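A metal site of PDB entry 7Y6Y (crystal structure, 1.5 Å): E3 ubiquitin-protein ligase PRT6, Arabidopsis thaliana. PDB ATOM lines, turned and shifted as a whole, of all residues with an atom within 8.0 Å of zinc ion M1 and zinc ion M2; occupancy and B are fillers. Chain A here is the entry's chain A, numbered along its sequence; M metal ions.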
ATOM      1  N   VAL A   8      19.337  26.485  -2.423  1.00  0.00           N
ATOM      2  CA  VAL A   8      20.381  25.558  -2.894  1.00  0.00           C
ATOM      3  C   VAL A   8      20.315  25.413  -4.423  1.00  0.00           C
ATOM      4  O   VAL A   8      19.240  25.346  -4.990  1.00  0.00           O
ATOM      5  CB  VAL A   8      20.272  24.188  -2.236  1.00  0.00           C
ATOM      6  CG1 VAL A   8      21.159  23.168  -2.963  1.00  0.00           C
ATOM      7  CG2 VAL A   8      20.680  24.253  -0.767  1.00  0.00           C
ATOM      8  N   CYS A   9      21.479  25.381  -5.063  1.00  0.00           N
ATOM      9  CA  CYS A   9      21.542  25.278  -6.511  1.00  0.00           C
ATOM     10  C   CYS A   9      20.930  23.970  -7.013  1.00  0.00           C
ATOM     11  O   CYS A   9      20.029  23.967  -7.850  1.00  0.00           O
ATOM     12  CB  CYS A   9      23.002  25.353  -6.974  1.00  0.00           C
ATOM     13  SG  CYS A   9      23.204  25.152  -8.815  1.00  0.00           S
ATOM     14  N   GLY A  10      21.511  22.854  -6.593  1.00  0.00           N
ATOM     15  CA  GLY A  10      20.997  21.524  -6.889  1.00  0.00           C
ATOM     16  C   GLY A  10      21.021  21.143  -8.376  1.00  0.00           C
ATOM     17  O   GLY A  10      20.415  20.133  -8.748  1.00  0.00           O
ATOM     18  N   SER A  11      21.677  21.938  -9.227  1.00  0.00           N
ATOM     19  CA  SER A  11      21.876  21.549 -10.626  1.00  0.00           C
ATOM     20  C   SER A  11      22.515  20.163 -10.717  1.00  0.00           C
ATOM     21  O   SER A  11      23.400  19.823  -9.944  1.00  0.00           O
ATOM     22  CB  SER A  11      22.809  22.537 -11.297  1.00  0.00           C
ATOM     23  OG  SER A  11      23.193  22.129 -12.587  1.00  0.00           O
ATOM     24  N   VAL A  12      22.143  19.423 -11.760  1.00  0.00           N
ATOM     25  CA  VAL A  12      22.462  17.988 -11.860  1.00  0.00           C
ATOM     26  C   VAL A  12      23.436  17.746 -13.003  1.00  0.00           C
ATOM     27  O   VAL A  12      23.300  18.302 -14.101  1.00  0.00           O
ATOM     28  CB  VAL A  12      21.199  17.116 -12.018  1.00  0.00           C
ATOM     29  CG1 VAL A  12      21.591  15.692 -12.458  1.00  0.00           C
ATOM     30  CG2 VAL A  12      20.409  17.073 -10.734  1.00  0.00           C
ATOM     31  N   TRP A  13      24.425  16.886 -12.735  1.00  0.00           N
ATOM     32  CA  TRP A  13      25.407  16.480 -13.723  1.00  0.00           C
ATOM     33  C   TRP A  13      25.099  15.082 -14.207  1.00  0.00           C
ATOM     34  O   TRP A  13      24.618  14.221 -13.468  1.00  0.00           O
ATOM     35  CB  TRP A  13      26.840  16.493 -13.174  1.00  0.00           C
ATOM     36  CG  TRP A  13      27.226  17.792 -12.623  1.00  0.00           C
ATOM     37  CD1 TRP A  13      27.258  18.981 -13.271  1.00  0.00           C
ATOM     38  CD2 TRP A  13      27.604  18.056 -11.270  1.00  0.00           C
ATOM     39  NE1 TRP A  13      27.619  19.985 -12.404  1.00  0.00           N
ATOM     40  CE2 TRP A  13      27.845  19.437 -11.168  1.00  0.00           C
ATOM     41  CE3 TRP A  13      27.750  17.259 -10.138  1.00  0.00           C
ATOM     42  CZ2 TRP A  13      28.236  20.040  -9.972  1.00  0.00           C
ATOM     43  CZ3 TRP A  13      28.137  17.855  -8.949  1.00  0.00           C
ATOM     44  CH2 TRP A  13      28.375  19.236  -8.875  1.00  0.00           C
ATOM     45  N   ALA A  32      31.055  19.081  -4.468  1.00  0.00           N
ATOM     46  CA  ALA A  32      31.433  19.756  -5.708  1.00  0.00           C
ATOM     47  C   ALA A  32      30.402  20.829  -6.067  1.00  0.00           C
ATOM     48  O   ALA A  32      29.249  20.807  -5.622  1.00  0.00           O
ATOM     49  CB  ALA A  32      31.583  18.763  -6.867  1.00  0.00           C
ATOM     50  N   ILE A  33      30.838  21.766  -6.885  1.00  0.00           N
ATOM     51  CA  ILE A  33      29.949  22.819  -7.338  1.00  0.00           C
ATOM     52  C   ILE A  33      30.047  22.944  -8.846  1.00  0.00           C
ATOM     53  O   ILE A  33      31.084  22.689  -9.469  1.00  0.00           O
ATOM     54  CB  ILE A  33      30.180  24.175  -6.663  1.00  0.00           C
ATOM     55  CG1 ILE A  33      31.577  24.736  -6.899  1.00  0.00           C
ATOM     56  CG2 ILE A  33      29.845  24.036  -5.155  1.00  0.00           C
ATOM     57  CD1 ILE A  33      31.594  26.190  -6.392  1.00  0.00           C
ATOM     58  N   CYS A  34      28.941  23.372  -9.442  1.00  0.00           N
ATOM     59  CA  CYS A  34      28.861  23.523 -10.888  1.00  0.00           C
ATOM     60  C   CYS A  34      29.728  24.690 -11.347  1.00  0.00           C
ATOM     61  O   CYS A  34      30.119  25.568 -10.571  1.00  0.00           O
ATOM     62  CB  CYS A  34      27.405  23.708 -11.360  1.00  0.00           C
ATOM     63  SG  CYS A  34      26.571  25.258 -10.924  1.00  0.00           S
ATOM     64  N   VAL A  35      30.034  24.685 -12.638  1.00  0.00           N
ATOM     65  CA  VAL A  35      30.901  25.708 -13.184  1.00  0.00           C
ATOM     66  C   VAL A  35      30.310  27.100 -13.021  1.00  0.00           C
ATOM     67  O   VAL A  35      31.037  28.016 -12.596  1.00  0.00           O
ATOM     68  CB  VAL A  35      31.253  25.388 -14.648  1.00  0.00           C
ATOM     69  CG1 VAL A  35      32.024  26.554 -15.293  1.00  0.00           C
ATOM     70  CG2 VAL A  35      32.066  24.098 -14.736  1.00  0.00           C
ATOM     71  N   PRO A  36      29.020  27.349 -13.304  1.00  0.00           N
ATOM     72  CA  PRO A  36      28.490  28.704 -13.065  1.00  0.00           C
ATOM     73  C   PRO A  36      28.613  29.159 -11.615  1.00  0.00           C
ATOM     74  O   PRO A  36      28.939  30.321 -11.349  1.00  0.00           O
ATOM     75  CB  PRO A  36      27.019  28.590 -13.495  1.00  0.00           C
ATOM     76  CG  PRO A  36      26.956  27.432 -14.430  1.00  0.00           C
ATOM     77  CD  PRO A  36      28.029  26.477 -13.983  1.00  0.00           C
ATOM     78  N   CYS A  37      28.328  28.273 -10.677  1.00  0.00           N
ATOM     79  CA  CYS A  37      28.477  28.622  -9.260  1.00  0.00           C
ATOM     80  C   CYS A  37      29.923  28.941  -8.925  1.00  0.00           C
ATOM     81  O   CYS A  37      30.199  29.898  -8.188  1.00  0.00           O
ATOM     82  CB  CYS A  37      27.948  27.481  -8.400  1.00  0.00           C
ATOM     83  SG  CYS A  37      26.081  27.532  -8.369  1.00  0.00           S
ATOM     84  N   PHE A  38      30.865  28.155  -9.458  1.00  0.00           N
ATOM     85  CA  PHE A  38      32.272  28.447  -9.225  1.00  0.00           C
ATOM     86  C   PHE A  38      32.636  29.824  -9.751  1.00  0.00           C
ATOM     87  O   PHE A  38      33.313  30.613  -9.083  1.00  0.00           O
ATOM     88  CB  PHE A  38      33.169  27.373  -9.876  1.00  0.00           C
ATOM     89  CG  PHE A  38      34.631  27.611  -9.637  1.00  0.00           C
ATOM     90  CD1 PHE A  38      35.229  27.161  -8.486  1.00  0.00           C
ATOM     91  CD2 PHE A  38      35.388  28.312 -10.562  1.00  0.00           C
ATOM     92  CE1 PHE A  38      36.592  27.402  -8.254  1.00  0.00           C
ATOM     93  CE2 PHE A  38      36.734  28.551 -10.363  1.00  0.00           C
ATOM     94  CZ  PHE A  38      37.323  28.098  -9.189  1.00  0.00           C
ATOM     95  N   ASN A  40      30.842  32.417 -10.200  1.00  0.00           N
ATOM     96  CA  ASN A  40      30.182  33.529  -9.542  1.00  0.00           C
ATOM     97  C   ASN A  40      30.498  33.573  -8.045  1.00  0.00           C
ATOM     98  O   ASN A  40      29.810  34.263  -7.308  1.00  0.00           O
ATOM     99  CB  ASN A  40      28.681  33.484  -9.795  1.00  0.00           C
ATOM    100  CG  ASN A  40      28.326  33.923 -11.198  1.00  0.00           C
ATOM    101  OD1 ASN A  40      28.136  33.114 -12.083  1.00  0.00           O
ATOM    102  ND2 ASN A  40      28.243  35.224 -11.406  1.00  0.00           N
ATOM    103  N   GLY A  41      31.527  32.845  -7.597  1.00  0.00           N
ATOM    104  CA  GLY A  41      32.014  32.925  -6.233  1.00  0.00           C
ATOM    105  C   GLY A  41      33.467  33.363  -6.185  1.00  0.00           C
ATOM    106  O   GLY A  41      34.025  33.743  -7.211  1.00  0.00           O
ATOM    107  N   CYS A  57      25.095  16.314  -7.970  1.00  0.00           N
ATOM    108  CA  CYS A  57      24.423  17.601  -7.961  1.00  0.00           C
ATOM    109  C   CYS A  57      25.265  18.654  -7.251  1.00  0.00           C
ATOM    110  O   CYS A  57      26.101  18.347  -6.393  1.00  0.00           O
ATOM    111  CB  CYS A  57      23.018  17.496  -7.349  1.00  0.00           C
ATOM    112  SG  CYS A  57      22.981  17.004  -5.623  1.00  0.00           S
ATOM    113  N   CYS A  58      25.025  19.911  -7.643  1.00  0.00           N
ATOM    114  CA  CYS A  58      25.807  21.023  -7.139  1.00  0.00           C
ATOM    115  C   CYS A  58      25.473  21.335  -5.678  1.00  0.00           C
ATOM    116  O   CYS A  58      24.303  21.424  -5.301  1.00  0.00           O
ATOM    117  CB  CYS A  58      25.542  22.264  -7.999  1.00  0.00           C
ATOM    118  SG  CYS A  58      26.380  23.704  -7.409  1.00  0.00           S
ATOM    119  N   ASP A  59      26.500  21.537  -4.866  1.00  0.00           N
ATOM    120  CA  ASP A  59      26.341  21.749  -3.425  1.00  0.00           C
ATOM    121  C   ASP A  59      26.238  23.224  -3.035  1.00  0.00           C
ATOM    122  O   ASP A  59      26.131  23.540  -1.830  1.00  0.00           O
ATOM    123  CB  ASP A  59      27.532  21.115  -2.693  1.00  0.00           C
ATOM    124  CG  ASP A  59      27.499  19.587  -2.741  1.00  0.00           C
ATOM    125  OD1 ASP A  59      26.393  19.023  -2.535  1.00  0.00           O
ATOM    126  OD2 ASP A  59      28.538  18.966  -3.038  1.00  0.00           O
ATOM    127  N   CYS A  60      26.284  24.126  -4.002  1.00  0.00           N
ATOM    128  CA  CYS A  60      26.367  25.555  -3.705  1.00  0.00           C
ATOM    129  C   CYS A  60      25.083  25.987  -3.036  1.00  0.00           C
ATOM    130  O   CYS A  60      23.992  25.647  -3.510  1.00  0.00           O
ATOM    131  CB  CYS A  60      26.561  26.353  -4.987  1.00  0.00           C
ATOM    132  SG  CYS A  60      26.747  28.115  -4.682  1.00  0.00           S
ATOM    133  N   GLY A  61      25.197  26.688  -1.912  1.00  0.00           N
ATOM    134  CA  GLY A  61      24.044  27.095  -1.113  1.00  0.00           C
ATOM    135  C   GLY A  61      23.676  26.155   0.016  1.00  0.00           C
ATOM    136  O   GLY A  61      22.874  26.539   0.876  1.00  0.00           O
ATOM    137  N   ASP A  62      24.266  24.960   0.070  1.00  0.00           N
ATOM    138  CA  ASP A  62      23.976  23.957   1.094  1.00  0.00           C
ATOM    139  C   ASP A  62      25.096  23.940   2.126  1.00  0.00           C
ATOM    140  O   ASP A  62      26.141  23.329   1.908  1.00  0.00           O
ATOM    141  CB  ASP A  62      23.807  22.590   0.424  1.00  0.00           C
ATOM    142  CG  ASP A  62      23.564  21.450   1.419  1.00  0.00           C
ATOM    143  OD1 ASP A  62      23.396  21.723   2.640  1.00  0.00           O
ATOM    144  OD2 ASP A  62      23.529  20.268   0.959  1.00  0.00           O
ATOM    145  N   TRP A  66      28.983  22.498   1.831  1.00  0.00           N
ATOM    146  CA  TRP A  66      29.895  23.511   1.314  1.00  0.00           C
ATOM    147  C   TRP A  66      29.960  24.680   2.298  1.00  0.00           C
ATOM    148  O   TRP A  66      28.931  25.074   2.871  1.00  0.00           O
ATOM    149  CB  TRP A  66      29.365  23.943  -0.056  1.00  0.00           C
ATOM    150  CG  TRP A  66      30.327  24.587  -0.997  1.00  0.00           C
ATOM    151  CD1 TRP A  66      30.489  25.922  -1.213  1.00  0.00           C
ATOM    152  CD2 TRP A  66      31.250  23.921  -1.849  1.00  0.00           C
ATOM    153  NE1 TRP A  66      31.469  26.134  -2.168  1.00  0.00           N
ATOM    154  CE2 TRP A  66      31.940  24.902  -2.569  1.00  0.00           C
ATOM    155  CE3 TRP A  66      31.541  22.575  -2.095  1.00  0.00           C
ATOM    156  CZ2 TRP A  66      32.912  24.586  -3.519  1.00  0.00           C
ATOM    157  CZ3 TRP A  66      32.491  22.258  -2.969  1.00  0.00           C
ATOM    158  CH2 TRP A  66      33.174  23.249  -3.695  1.00  0.00           C
ATOM    159  N   GLY A  70      32.155  30.009   0.428  1.00  0.00           N
ATOM    160  CA  GLY A  70      32.311  29.473  -0.908  1.00  0.00           C
ATOM    161  C   GLY A  70      31.067  29.493  -1.750  1.00  0.00           C
ATOM    162  O   GLY A  70      31.096  29.029  -2.901  1.00  0.00           O
ATOM    163  N   PHE A  71      29.961  30.032  -1.229  1.00  0.00           N
ATOM    164  CA  PHE A  71      28.732  30.165  -2.008  1.00  0.00           C
ATOM    165  C   PHE A  71      28.873  31.244  -3.067  1.00  0.00           C
ATOM    166  O   PHE A  71      29.609  32.218  -2.900  1.00  0.00           O
ATOM    167  CB  PHE A  71      27.561  30.553  -1.121  1.00  0.00           C
ATOM    168  CG  PHE A  71      27.123  29.503  -0.146  1.00  0.00           C
ATOM    169  CD1 PHE A  71      26.171  29.834   0.822  1.00  0.00           C
ATOM    170  CD2 PHE A  71      27.643  28.219  -0.147  1.00  0.00           C
ATOM    171  CE1 PHE A  71      25.717  28.895   1.743  1.00  0.00           C
ATOM    172  CE2 PHE A  71      27.182  27.268   0.760  1.00  0.00           C
ATOM    173  CZ  PHE A  71      26.229  27.605   1.707  1.00  0.00           C
ATOM    174  N   CYS A  72      28.158  31.070  -4.147  1.00  0.00           N
ATOM    175  CA  CYS A  72      28.137  32.080  -5.210  1.00  0.00           C
ATOM    176  C   CYS A  72      27.112  33.152  -4.877  1.00  0.00           C
ATOM    177  O   CYS A  72      26.301  33.018  -3.976  1.00  0.00           O
ATOM    178  CB  CYS A  72      27.821  31.452  -6.561  1.00  0.00           C
ATOM    179  SG  CYS A  72      26.079  31.172  -6.929  1.00  0.00           S
ATOM    180  N   SER A  73      27.114  34.204  -5.693  1.00  0.00           N
ATOM    181  CA  SER A  73      26.275  35.370  -5.423  1.00  0.00           C
ATOM    182  C   SER A  73      24.782  35.081  -5.578  1.00  0.00           C
ATOM    183  O   SER A  73      23.961  35.889  -5.106  1.00  0.00           O
ATOM    184  CB  SER A  73      26.691  36.508  -6.365  1.00  0.00           C
ATOM    185  OG  SER A  73      26.612  36.094  -7.714  1.00  0.00           O
ATOM    186  N   ASN A  74      24.407  33.981  -6.194  1.00  0.00           N
ATOM    187  CA  ASN A  74      23.020  33.628  -6.409  1.00  0.00           C
ATOM    188  C   ASN A  74      22.457  32.674  -5.364  1.00  0.00           C
ATOM    189  O   ASN A  74      21.239  32.471  -5.339  1.00  0.00           O
ATOM    190  CB  ASN A  74      22.830  32.998  -7.800  1.00  0.00           C
ATOM    191  CG  ASN A  74      23.106  33.954  -8.922  1.00  0.00           C
ATOM    192  OD1 ASN A  74      23.721  33.573  -9.933  1.00  0.00           O
ATOM    193  ND2 ASN A  74      22.680  35.199  -8.771  1.00  0.00           N
ATOM    194  N   HIS A  75      23.291  32.124  -4.478  1.00  0.00           N
ATOM    195  CA  HIS A  75      22.826  31.123  -3.521  1.00  0.00           C
ATOM    196  C   HIS A  75      23.251  31.470  -2.095  1.00  0.00           C
ATOM    197  O   HIS A  75      23.490  30.586  -1.264  1.00  0.00           O
ATOM    198  CB  HIS A  75      23.338  29.734  -3.929  1.00  0.00           C
ATOM    199  CG  HIS A  75      22.828  29.312  -5.263  1.00  0.00           C
ATOM    200  ND1 HIS A  75      23.645  29.094  -6.353  1.00  0.00           N
ATOM    201  CD2 HIS A  75      21.556  29.158  -5.723  1.00  0.00           C
ATOM    202  CE1 HIS A  75      22.913  28.798  -7.410  1.00  0.00           C
ATOM    203  NE2 HIS A  75      21.639  28.830  -7.053  1.00  0.00           N
ATOM    204  N   LYS A  76      23.280  32.763  -1.769  1.00  0.00           N
ATOM    205  CA  LYS A  76      23.593  33.208  -0.419  1.00  0.00           C
ATOM    206  C   LYS A  76      22.310  33.596   0.306  1.00  0.00           C
ATOM    207  O   LYS A  76      22.328  33.713   1.527  1.00  0.00           O
ATOM    208  CB  LYS A  76      24.548  34.377  -0.449  1.00  0.00           C
ATOM    209  CG  LYS A  76      25.946  34.012  -0.855  1.00  0.00           C
ATOM    210  CD  LYS A  76      26.831  35.223  -0.673  1.00  0.00           C
ATOM    211  CE  LYS A  76      28.095  35.050  -1.416  1.00  0.00           C
ATOM    212  NZ  LYS A  76      29.117  36.039  -1.006  1.00  0.00           N
HETATM  213 ZN    ZN M   1      25.516  25.296  -8.870  1.00  0.00          ZN
HETATM  214 ZN    ZN M   2      25.621  28.939  -6.452  1.00  0.00          ZN
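N of Cys 9 sits at hydrogen-bond distance from O of Cys 60, at 3.0 Å.
The backbone NH of Cys 60 sits close to the side-chain sulfur of Cys 58 (3.4 Å).
SG of Cys 9 sits close to N of Ser 11 (3.6 Å).
The backbone carbonyl oxygen (O) of Ser 11 sits at hydrogen-bond distance from the backbone NH (N) of Cys 58, 2.8 Å away.
N of Gly 10 is in hydrogen-bond range of O of Cys 58, at 3.4 Å.
The side-chain sulfur (SG) of Cys 72 sits close to the backbone NH (N) of Asn 74, at 3.4 Å.
Within 4 Å of zinc ion M2: Cys 37, Cys 60, Cys 72 and His 75.
The nearest printed residue that does not touch zinc ion M2 is Cys 9 (4.5 Å).
SG of Cys 34 is bound to zinc ion M1, at 2.3 Å.
Zinc ion M1 is bound by SG of Cys 9, at 2.3 Å.
Zinc ion M1 is bound by SG of Cys 58, 2.3 Å away.
SG of Cys 37 binds zinc ion M1 (2.4 Å).
Zinc ion M2 is bound by ND1 of His 75 (2.0 Å), SG of Cys 60 (2.3 Å), SG of Cys 72 (2.3 Å) and SG of Cys 37 (2.4 Å).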
